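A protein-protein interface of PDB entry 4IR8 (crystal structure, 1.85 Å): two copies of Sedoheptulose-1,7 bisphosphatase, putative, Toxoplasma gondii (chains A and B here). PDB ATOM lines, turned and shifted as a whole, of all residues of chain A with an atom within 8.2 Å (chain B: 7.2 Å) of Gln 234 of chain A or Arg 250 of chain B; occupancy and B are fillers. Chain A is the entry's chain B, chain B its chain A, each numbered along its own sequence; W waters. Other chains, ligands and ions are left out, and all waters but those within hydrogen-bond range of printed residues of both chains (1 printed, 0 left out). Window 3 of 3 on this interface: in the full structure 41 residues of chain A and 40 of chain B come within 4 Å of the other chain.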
ATOM      1  N   ASN A 229       2.643 -27.514  -5.134  1.00  0.00           N
ATOM      2  CA  ASN A 229       3.272 -28.697  -4.545  1.00  0.00           C
ATOM      3  C   ASN A 229       4.703 -28.351  -4.108  1.00  0.00           C
ATOM      4  O   ASN A 229       5.655 -29.107  -4.338  1.00  0.00           O
ATOM      5  CB  ASN A 229       3.290 -29.840  -5.568  1.00  0.00           C
ATOM      6  CG  ASN A 229       3.501 -31.201  -4.927  1.00  0.00           C
ATOM      7  OD1 ASN A 229       3.168 -31.401  -3.756  1.00  0.00           O
ATOM      8  ND2 ASN A 229       4.028 -32.148  -5.696  1.00  0.00           N
ATOM      9  N   LEU A 230       4.835 -27.190  -3.485  1.00  0.00           N
ATOM     10  CA  LEU A 230       6.121 -26.641  -3.072  1.00  0.00           C
ATOM     11  C   LEU A 230       6.961 -27.636  -2.279  1.00  0.00           C
ATOM     12  O   LEU A 230       8.192 -27.687  -2.445  1.00  0.00           O
ATOM     13  CB  LEU A 230       5.898 -25.369  -2.256  1.00  0.00           C
ATOM     14  CG  LEU A 230       7.131 -24.557  -1.877  1.00  0.00           C
ATOM     15  CD1 LEU A 230       7.894 -24.098  -3.119  1.00  0.00           C
ATOM     16  CD2 LEU A 230       6.710 -23.359  -1.017  1.00  0.00           C
ATOM     17  N   ARG A 231       6.302 -28.432  -1.435  1.00  0.00           N
ATOM     18  CA  ARG A 231       6.994 -29.440  -0.624  1.00  0.00           C
ATOM     19  C   ARG A 231       7.816 -30.432  -1.435  1.00  0.00           C
ATOM     20  O   ARG A 231       8.758 -31.020  -0.902  1.00  0.00           O
ATOM     21  CB  ARG A 231       6.019 -30.207   0.298  1.00  0.00           C
ATOM     22  CG  ARG A 231       4.839 -30.868  -0.382  1.00  0.00           C
ATOM     23  CD  ARG A 231       3.851 -31.465   0.654  1.00  0.00           C
ATOM     24  NE  ARG A 231       4.241 -32.812   1.085  1.00  0.00           N
ATOM     25  CZ  ARG A 231       3.682 -33.945   0.652  1.00  0.00           C
ATOM     26  NH1 ARG A 231       2.662 -33.928  -0.208  1.00  0.00           N
ATOM     27  NH2 ARG A 231       4.128 -35.109   1.101  1.00  0.00           N
ATOM     28  N   ALA A 232       7.460 -30.633  -2.705  1.00  0.00           N
ATOM     29  CA  ALA A 232       8.207 -31.541  -3.581  1.00  0.00           C
ATOM     30  C   ALA A 232       9.662 -31.064  -3.750  1.00  0.00           C
ATOM     31  O   ALA A 232      10.558 -31.876  -3.979  1.00  0.00           O
ATOM     32  CB  ALA A 232       7.525 -31.647  -4.939  1.00  0.00           C
ATOM     33  N   ALA A 233       9.880 -29.754  -3.640  1.00  0.00           N
ATOM     34  CA  ALA A 233      11.230 -29.165  -3.775  1.00  0.00           C
ATOM     35  C   ALA A 233      12.204 -29.732  -2.745  1.00  0.00           C
ATOM     36  O   ALA A 233      13.425 -29.823  -2.997  1.00  0.00           O
ATOM     37  CB  ALA A 233      11.151 -27.637  -3.652  1.00  0.00           C
ATOM     38  N   GLN A 234      11.667 -30.153  -1.602  1.00  0.00           N
ATOM     39  CA  GLN A 234      12.494 -30.703  -0.535  1.00  0.00           C
ATOM     40  C   GLN A 234      13.111 -32.074  -0.865  1.00  0.00           C
ATOM     41  O   GLN A 234      14.079 -32.468  -0.231  1.00  0.00           O
ATOM     42  CB  GLN A 234      11.730 -30.704   0.795  1.00  0.00           C
ATOM     43  CG  GLN A 234      11.320 -29.289   1.239  1.00  0.00           C
ATOM     44  CD  GLN A 234      12.499 -28.314   1.322  1.00  0.00           C
ATOM     45  OE1 GLN A 234      13.555 -28.627   1.896  1.00  0.00           O
ATOM     46  NE2 GLN A 234      12.326 -27.127   0.738  1.00  0.00           N
ATOM     47  N   ASP A 235      12.570 -32.795  -1.847  1.00  0.00           N
ATOM     48  CA  ASP A 235      13.211 -34.048  -2.283  1.00  0.00           C
ATOM     49  C   ASP A 235      13.329 -34.115  -3.807  1.00  0.00           C
ATOM     50  O   ASP A 235      13.468 -35.195  -4.374  1.00  0.00           O
ATOM     51  CB  ASP A 235      12.543 -35.320  -1.705  1.00  0.00           C
ATOM     52  CG  ASP A 235      11.176 -35.616  -2.307  1.00  0.00           C
ATOM     53  OD1 ASP A 235      10.910 -36.804  -2.625  1.00  0.00           O
ATOM     54  OD2 ASP A 235      10.368 -34.686  -2.462  1.00  0.00           O
ATOM     55  N   LEU A 236      13.306 -32.949  -4.450  1.00  0.00           N
ATOM     56  CA  LEU A 236      13.456 -32.830  -5.896  1.00  0.00           C
ATOM     57  C   LEU A 236      14.388 -31.612  -6.136  1.00  0.00           C
ATOM     58  O   LEU A 236      13.925 -30.476  -6.301  1.00  0.00           O
ATOM     59  CB  LEU A 236      12.093 -32.642  -6.552  1.00  0.00           C
ATOM     60  CG  LEU A 236      11.987 -32.879  -8.054  1.00  0.00           C
ATOM     61  CD1 LEU A 236      12.279 -34.341  -8.385  1.00  0.00           C
ATOM     62  CD2 LEU A 236      10.613 -32.496  -8.556  1.00  0.00           C
ATOM     63  N   PRO A 237      15.709 -31.851  -6.132  1.00  0.00           N
ATOM     64  CA  PRO A 237      16.692 -30.767  -6.265  1.00  0.00           C
ATOM     65  C   PRO A 237      16.462 -29.805  -7.426  1.00  0.00           C
ATOM     66  O   PRO A 237      16.634 -28.596  -7.251  1.00  0.00           O
ATOM     67  CB  PRO A 237      18.012 -31.512  -6.451  1.00  0.00           C
ATOM     68  CG  PRO A 237      17.795 -32.816  -5.783  1.00  0.00           C
ATOM     69  CD  PRO A 237      16.363 -33.162  -5.937  1.00  0.00           C
ATOM     70  N   TYR A 239      13.722 -28.847  -8.867  1.00  0.00           N
ATOM     71  CA  TYR A 239      12.622 -27.929  -8.552  1.00  0.00           C
ATOM     72  C   TYR A 239      13.075 -26.903  -7.518  1.00  0.00           C
ATOM     73  O   TYR A 239      12.837 -25.694  -7.674  1.00  0.00           O
ATOM     74  CB  TYR A 239      11.398 -28.710  -8.072  1.00  0.00           C
ATOM     75  CG  TYR A 239      10.115 -27.896  -7.926  1.00  0.00           C
ATOM     76  CD1 TYR A 239       9.774 -26.918  -8.856  1.00  0.00           C
ATOM     77  CD2 TYR A 239       9.193 -28.190  -6.931  1.00  0.00           C
ATOM     78  CE1 TYR A 239       8.591 -26.194  -8.751  1.00  0.00           C
ATOM     79  CE2 TYR A 239       7.975 -27.466  -6.826  1.00  0.00           C
ATOM     80  CZ  TYR A 239       7.689 -26.486  -7.757  1.00  0.00           C
ATOM     81  OH  TYR A 239       6.517 -25.761  -7.701  1.00  0.00           O
ATOM     82  N   LYS A 240      13.790 -27.369  -6.493  1.00  0.00           N
ATOM     83  CA  LYS A 240      14.341 -26.457  -5.506  1.00  0.00           C
ATOM     84  C   LYS A 240      15.230 -25.402  -6.179  1.00  0.00           C
ATOM     85  O   LYS A 240      15.108 -24.214  -5.899  1.00  0.00           O
ATOM     86  CB  LYS A 240      15.130 -27.217  -4.447  1.00  0.00           C
ATOM     87  CG  LYS A 240      15.690 -26.346  -3.329  1.00  0.00           C
ATOM     88  CD  LYS A 240      14.587 -25.695  -2.520  1.00  0.00           C
ATOM     89  CE  LYS A 240      15.159 -25.004  -1.275  1.00  0.00           C
ATOM     90  NZ  LYS A 240      14.068 -24.427  -0.463  1.00  0.00           N
ATOM     91  N   ILE A 243      13.179 -22.858  -8.283  1.00  0.00           N
ATOM     92  CA  ILE A 243      12.539 -21.901  -7.366  1.00  0.00           C
ATOM     93  C   ILE A 243      13.565 -20.875  -6.852  1.00  0.00           C
ATOM     94  O   ILE A 243      13.295 -19.670  -6.825  1.00  0.00           O
ATOM     95  CB  ILE A 243      11.875 -22.624  -6.198  1.00  0.00           C
ATOM     96  CG1 ILE A 243      10.673 -23.405  -6.709  1.00  0.00           C
ATOM     97  CG2 ILE A 243      11.439 -21.643  -5.129  1.00  0.00           C
ATOM     98  CD1 ILE A 243      10.149 -24.407  -5.717  1.00  0.00           C
ATOM     99  N   GLU A 244      14.746 -21.350  -6.471  1.00  0.00           N
ATOM    100  CA  GLU A 244      15.807 -20.442  -6.030  1.00  0.00           C
ATOM    101  C   GLU A 244      16.192 -19.475  -7.143  1.00  0.00           C
ATOM    102  O   GLU A 244      16.415 -18.278  -6.894  1.00  0.00           O
ATOM    103  CB  GLU A 244      17.036 -21.236  -5.562  1.00  0.00           C
ATOM    104  CG  GLU A 244      16.761 -22.072  -4.325  1.00  0.00           C
ATOM    105  CD  GLU A 244      16.555 -21.250  -3.067  1.00  0.00           C
ATOM    106  OE1 GLU A 244      17.052 -20.099  -2.997  1.00  0.00           O
ATOM    107  OE2 GLU A 244      15.915 -21.778  -2.127  1.00  0.00           O
ATOM    108  N   SER A 279       7.260 -35.592  -6.947  1.00  0.00           N
ATOM    109  CA  SER A 279       8.463 -36.138  -6.307  1.00  0.00           C
ATOM    110  C   SER A 279       8.048 -37.429  -5.626  1.00  0.00           C
ATOM    111  O   SER A 279       6.852 -37.729  -5.527  1.00  0.00           O
ATOM    112  CB  SER A 279       9.052 -35.182  -5.265  1.00  0.00           C
ATOM    113  OG  SER A 279       8.288 -35.190  -4.067  1.00  0.00           O
ATOM    114  N   ALA A 281       8.331 -38.154  -2.435  1.00  0.00           N
ATOM    115  CA  ALA A 281       7.682 -37.752  -1.181  1.00  0.00           C
ATOM    116  C   ALA A 281       6.355 -37.018  -1.390  1.00  0.00           C
ATOM    117  O   ALA A 281       5.438 -37.142  -0.581  1.00  0.00           O
ATOM    118  CB  ALA A 281       8.641 -36.860  -0.371  1.00  0.00           C
ATOM    119  N   ALA A 282       6.275 -36.243  -2.465  1.00  0.00           N
ATOM    120  CA  ALA A 282       5.086 -35.448  -2.775  1.00  0.00           C
ATOM    121  C   ALA A 282       4.644 -35.749  -4.203  1.00  0.00           C
ATOM    122  O   ALA A 282       4.953 -35.001  -5.123  1.00  0.00           O
ATOM    123  CB  ALA A 282       5.399 -33.964  -2.619  1.00  0.00           C
ATOM    124  N   LYS B 223       0.652 -22.791  10.005  1.00  0.00           N
ATOM    125  CA  LYS B 223       0.934 -23.751   8.966  1.00  0.00           C
ATOM    126  C   LYS B 223       1.168 -23.010   7.649  1.00  0.00           C
ATOM    127  O   LYS B 223       1.989 -23.418   6.854  1.00  0.00           O
ATOM    128  CB  LYS B 223      -0.211 -24.760   8.836  1.00  0.00           C
ATOM    129  CG  LYS B 223      -0.330 -25.697  10.042  1.00  0.00           C
ATOM    130  CD  LYS B 223       0.897 -26.613  10.160  1.00  0.00           C
ATOM    131  CE  LYS B 223       0.767 -27.611  11.295  1.00  0.00           C
ATOM    132  NZ  LYS B 223       1.933 -28.530  11.337  1.00  0.00           N
ATOM    133  N   PHE B 225       2.300 -19.711   5.292  1.00  0.00           N
ATOM    134  CA  PHE B 225       3.152 -18.525   5.230  1.00  0.00           C
ATOM    135  C   PHE B 225       2.850 -17.771   3.941  1.00  0.00           C
ATOM    136  O   PHE B 225       2.556 -18.370   2.925  1.00  0.00           O
ATOM    137  CB  PHE B 225       4.640 -18.837   5.383  1.00  0.00           C
ATOM    138  CG  PHE B 225       5.300 -19.478   4.168  1.00  0.00           C
ATOM    139  CD1 PHE B 225       6.232 -18.768   3.430  1.00  0.00           C
ATOM    140  CD2 PHE B 225       5.034 -20.794   3.816  1.00  0.00           C
ATOM    141  CE1 PHE B 225       6.905 -19.362   2.356  1.00  0.00           C
ATOM    142  CE2 PHE B 225       5.681 -21.387   2.739  1.00  0.00           C
ATOM    143  CZ  PHE B 225       6.616 -20.662   2.000  1.00  0.00           C
ATOM    144  N   ILE B 243      12.282 -17.582   4.959  1.00  0.00           N
ATOM    145  CA  ILE B 243      11.567 -18.218   3.868  1.00  0.00           C
ATOM    146  C   ILE B 243      12.113 -19.637   3.634  1.00  0.00           C
ATOM    147  O   ILE B 243      11.351 -20.575   3.444  1.00  0.00           O
ATOM    148  CB  ILE B 243      11.710 -17.396   2.588  1.00  0.00           C
ATOM    149  CG1 ILE B 243      10.973 -16.072   2.759  1.00  0.00           C
ATOM    150  CG2 ILE B 243      11.193 -18.196   1.364  1.00  0.00           C
ATOM    151  CD1 ILE B 243      11.276 -15.067   1.708  1.00  0.00           C
ATOM    152  N   GLU B 244      13.434 -19.791   3.646  1.00  0.00           N
ATOM    153  CA  GLU B 244      14.038 -21.115   3.442  1.00  0.00           C
ATOM    154  C   GLU B 244      13.598 -22.060   4.546  1.00  0.00           C
ATOM    155  O   GLU B 244      13.298 -23.222   4.298  1.00  0.00           O
ATOM    156  CB  GLU B 244      15.565 -21.042   3.387  1.00  0.00           C
ATOM    157  CG  GLU B 244      16.113 -20.355   2.160  1.00  0.00           C
ATOM    158  CD  GLU B 244      15.818 -21.109   0.869  1.00  0.00           C
ATOM    159  OE1 GLU B 244      15.775 -22.370   0.875  1.00  0.00           O
ATOM    160  OE2 GLU B 244      15.640 -20.420  -0.161  1.00  0.00           O
ATOM    161  N   PHE B 245      13.554 -21.554   5.769  1.00  0.00           N
ATOM    162  CA  PHE B 245      13.107 -22.348   6.902  1.00  0.00           C
ATOM    163  C   PHE B 245      11.646 -22.797   6.708  1.00  0.00           C
ATOM    164  O   PHE B 245      11.330 -23.988   6.847  1.00  0.00           O
ATOM    165  CB  PHE B 245      13.271 -21.544   8.197  1.00  0.00           C
ATOM    166  CG  PHE B 245      12.653 -22.192   9.397  1.00  0.00           C
ATOM    167  CD1 PHE B 245      13.349 -23.149  10.124  1.00  0.00           C
ATOM    168  CD2 PHE B 245      11.368 -21.851   9.798  1.00  0.00           C
ATOM    169  CE1 PHE B 245      12.769 -23.753  11.246  1.00  0.00           C
ATOM    170  CE2 PHE B 245      10.789 -22.443  10.921  1.00  0.00           C
ATOM    171  CZ  PHE B 245      11.477 -23.405  11.627  1.00  0.00           C
ATOM    172  N   TRP B 246      10.773 -21.862   6.357  1.00  0.00           N
ATOM    173  CA  TRP B 246       9.371 -22.197   6.137  1.00  0.00           C
ATOM    174  C   TRP B 246       9.214 -23.262   5.076  1.00  0.00           C
ATOM    175  O   TRP B 246       8.406 -24.148   5.208  1.00  0.00           O
ATOM    176  CB  TRP B 246       8.516 -20.967   5.814  1.00  0.00           C
ATOM    177  CG  TRP B 246       8.326 -20.058   6.963  1.00  0.00           C
ATOM    178  CD1 TRP B 246       8.159 -20.418   8.279  1.00  0.00           C
ATOM    179  CD2 TRP B 246       8.191 -18.625   6.920  1.00  0.00           C
ATOM    180  NE1 TRP B 246       7.976 -19.291   9.053  1.00  0.00           N
ATOM    181  CE2 TRP B 246       7.979 -18.185   8.244  1.00  0.00           C
ATOM    182  CE3 TRP B 246       8.252 -17.670   5.896  1.00  0.00           C
ATOM    183  CZ2 TRP B 246       7.825 -16.838   8.566  1.00  0.00           C
ATOM    184  CZ3 TRP B 246       8.103 -16.330   6.226  1.00  0.00           C
ATOM    185  CH2 TRP B 246       7.885 -15.932   7.539  1.00  0.00           C
ATOM    186  N   MET B 247      10.007 -23.168   4.019  1.00  0.00           N
ATOM    187  CA  MET B 247       9.971 -24.165   2.964  1.00  0.00           C
ATOM    188  C   MET B 247      10.487 -25.516   3.456  1.00  0.00           C
ATOM    189  O   MET B 247       9.864 -26.553   3.217  1.00  0.00           O
ATOM    190  CB  MET B 247      10.801 -23.683   1.777  1.00  0.00           C
ATOM    191  CG  MET B 247      10.191 -22.490   1.090  1.00  0.00           C
ATOM    192  SD  MET B 247      11.221 -21.850  -0.235  1.00  0.00           S
ATOM    193  CE  MET B 247      11.307 -23.294  -1.297  1.00  0.00           C
ATOM    194  N   GLU B 248      11.615 -25.500   4.158  1.00  0.00           N
ATOM    195  CA  GLU B 248      12.235 -26.748   4.684  1.00  0.00           C
ATOM    196  C   GLU B 248      11.332 -27.471   5.684  1.00  0.00           C
ATOM    197  O   GLU B 248      11.331 -28.705   5.760  1.00  0.00           O
ATOM    198  CB  GLU B 248      13.608 -26.444   5.308  1.00  0.00           C
ATOM    199  CG  GLU B 248      14.657 -26.026   4.269  1.00  0.00           C
ATOM    200  CD  GLU B 248      15.888 -25.370   4.877  1.00  0.00           C
ATOM    201  OE1 GLU B 248      16.829 -25.066   4.109  1.00  0.00           O
ATOM    202  OE2 GLU B 248      15.907 -25.141   6.108  1.00  0.00           O
ATOM    203  N   LYS B 249      10.564 -26.701   6.444  1.00  0.00           N
ATOM    204  CA  LYS B 249       9.626 -27.244   7.431  1.00  0.00           C
ATOM    205  C   LYS B 249       8.233 -27.550   6.842  1.00  0.00           C
ATOM    206  O   LYS B 249       7.301 -27.899   7.567  1.00  0.00           O
ATOM    207  CB  LYS B 249       9.529 -26.316   8.636  1.00  0.00           C
ATOM    208  CG  LYS B 249      10.760 -26.366   9.541  1.00  0.00           C
ATOM    209  CD  LYS B 249      10.774 -27.669  10.307  1.00  0.00           C
ATOM    210  CE  LYS B 249      12.018 -27.840  11.112  1.00  0.00           C
ATOM    211  NZ  LYS B 249      11.984 -29.137  11.837  1.00  0.00           N
ATOM    212  N   ARG B 250       8.114 -27.382   5.528  1.00  0.00           N
ATOM    213  CA  ARG B 250       6.899 -27.705   4.780  1.00  0.00           C
ATOM    214  C   ARG B 250       5.659 -26.920   5.180  1.00  0.00           C
ATOM    215  O   ARG B 250       4.549 -27.462   5.236  1.00  0.00           O
ATOM    216  CB  ARG B 250       6.655 -29.212   4.806  1.00  0.00           C
ATOM    217  CG  ARG B 250       7.860 -29.968   4.249  1.00  0.00           C
ATOM    218  CD  ARG B 250       7.667 -31.463   4.206  1.00  0.00           C
ATOM    219  NE  ARG B 250       8.832 -32.107   3.614  1.00  0.00           N
ATOM    220  CZ  ARG B 250       9.901 -32.490   4.301  1.00  0.00           C
ATOM    221  NH1 ARG B 250       9.950 -32.307   5.614  1.00  0.00           N
ATOM    222  NH2 ARG B 250      10.916 -33.062   3.676  1.00  0.00           N
ATOM    223  N   TYR B 251       5.858 -25.634   5.446  1.00  0.00           N
ATOM    224  CA  TYR B 251       4.742 -24.726   5.724  1.00  0.00           C
ATOM    225  C   TYR B 251       4.033 -24.606   4.375  1.00  0.00           C
ATOM    226  O   TYR B 251       4.616 -24.880   3.318  1.00  0.00           O
ATOM    227  CB  TYR B 251       5.194 -23.346   6.194  1.00  0.00           C
ATOM    228  CG  TYR B 251       5.669 -23.252   7.644  1.00  0.00           C
ATOM    229  CD1 TYR B 251       6.834 -23.877   8.066  1.00  0.00           C
ATOM    230  CD2 TYR B 251       4.987 -22.467   8.564  1.00  0.00           C
ATOM    231  CE1 TYR B 251       7.278 -23.767   9.390  1.00  0.00           C
ATOM    232  CE2 TYR B 251       5.416 -22.352   9.874  1.00  0.00           C
ATOM    233  CZ  TYR B 251       6.558 -22.994  10.286  1.00  0.00           C
ATOM    234  OH  TYR B 251       6.985 -22.846  11.588  1.00  0.00           O
ATOM    235  N   THR B 252       2.759 -24.251   4.416  1.00  0.00           N
ATOM    236  CA  THR B 252       1.964 -24.150   3.203  1.00  0.00           C
ATOM    237  C   THR B 252       2.036 -22.733   2.632  1.00  0.00           C
ATOM    238  O   THR B 252       1.753 -21.766   3.323  1.00  0.00           O
ATOM    239  CB  THR B 252       0.515 -24.532   3.481  1.00  0.00           C
ATOM    240  OG1 THR B 252       0.462 -25.901   3.893  1.00  0.00           O
ATOM    241  CG2 THR B 252      -0.370 -24.343   2.237  1.00  0.00           C
ATOM    242  N   LEU B 253       2.442 -22.609   1.371  1.00  0.00           N
ATOM    243  CA  LEU B 253       2.535 -21.274   0.734  1.00  0.00           C
ATOM    244  C   LEU B 253       1.182 -20.796   0.207  1.00  0.00           C
ATOM    245  O   LEU B 253       0.525 -21.513  -0.541  1.00  0.00           O
ATOM    246  CB  LEU B 253       3.510 -21.329  -0.452  1.00  0.00           C
ATOM    247  CG  LEU B 253       3.631 -20.055  -1.290  1.00  0.00           C
ATOM    248  CD1 LEU B 253       4.235 -18.917  -0.456  1.00  0.00           C
ATOM    249  CD2 LEU B 253       4.456 -20.328  -2.571  1.00  0.00           C
HETATM  250  O   HOH W   1       7.035 -33.455   1.238  1.00  0.00           O
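OE1 of Glu 244 of chain B is in salt-bridge range of NZ of Lys 240 of chain A (3.0 Å).
The side-chain carboxylate of Glu 244 of chain A lies close to the side-chain carboxylate of Glu 244 of chain B, at 2.4 Å.
Of the printed residues of chain B, Gln 234 of chain A touches Met 247, Glu 248 and Arg 250.
Printed residues of chain A within 4 Å of Arg 250 of chain B: Gln 234 (3.8 Å).
Of the printed residues of chain A, Glu 248 of chain B touches Gln 234 (3.6 Å).
Printed residues of chain B within 4 Å of Leu 230 of chain A: Met 247 (3.95 Å) and Leu 253 (3.8 Å).
Of the printed residues of chain A, Met 247 of chain B touches Leu 230, Gln 234 and Lys 240.
Printed residues of chain A within 4 Å of Leu 253 of chain B: Leu 230 (3.8 Å).
Ser 279 of chain A touches none of the printed residues of chain B.
Ala 232 of chain A touches none of the printed residues of chain B.
The nearest printed residue of chain A that does not touch Arg 250 of chain B is Arg 231 of chain A (4.4 Å).
Water W1 bridges the guanidinium group of Arg 231 of chain A (2.9 Å) and the guanidinium group of Arg 250 of chain B (3.3 Å).
Glu 244 of chain B touches its own counterpart, Glu 244 of chain A.
Of the 8 pairs that touch across the chains among the printed residues, 1 has its exchanged pair printed and touching as well.
Of the 13 printed residues of chain B, 5 touch a printed residue of chain A.
Printed residues of chain B that touch a printed residue of chain A: Glu 244, Met 247, Glu 248, Arg 250 and Leu 253.
Hydrophobic or aromatic side chains of chain A within 4 Å of the printed part of chain B: Leu 230.
Among the printed residues, Asp or Glu carboxylates within 4 Å of a Lys or Arg side-chain nitrogen of the other chain: Lys 240 of chain A with Glu 244 of chain B (3.0 Å).
The side-chain amino group of Lys 240 of chain A sits close to the side-chain amide nitrogen of Gln 234 of chain A, 3.4 Å away.
OE2 of Glu 244 of chain A lies within salt-bridge range of NZ of Lys 240 of chain A (3.6 Å).
Met 247 of chain B touches Leu 230 of chain A (CE to CD1, 3.95 Å).
Leu 230 of chain A touches Leu 253 of chain B.
Gln 234 of chain A touches Met 247 of chain B (NE2 to O, 3.5 Å).
OE1 of Gln 234 of chain A touches CA of Glu 248 of chain B, at 3.6 Å.
Gln 234 of chain A touches Arg 250 of chain B (CB to NH2, 3.8 Å).
Lys 240 of chain A touches Met 247 of chain B (NZ to CE, 3.1 Å).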
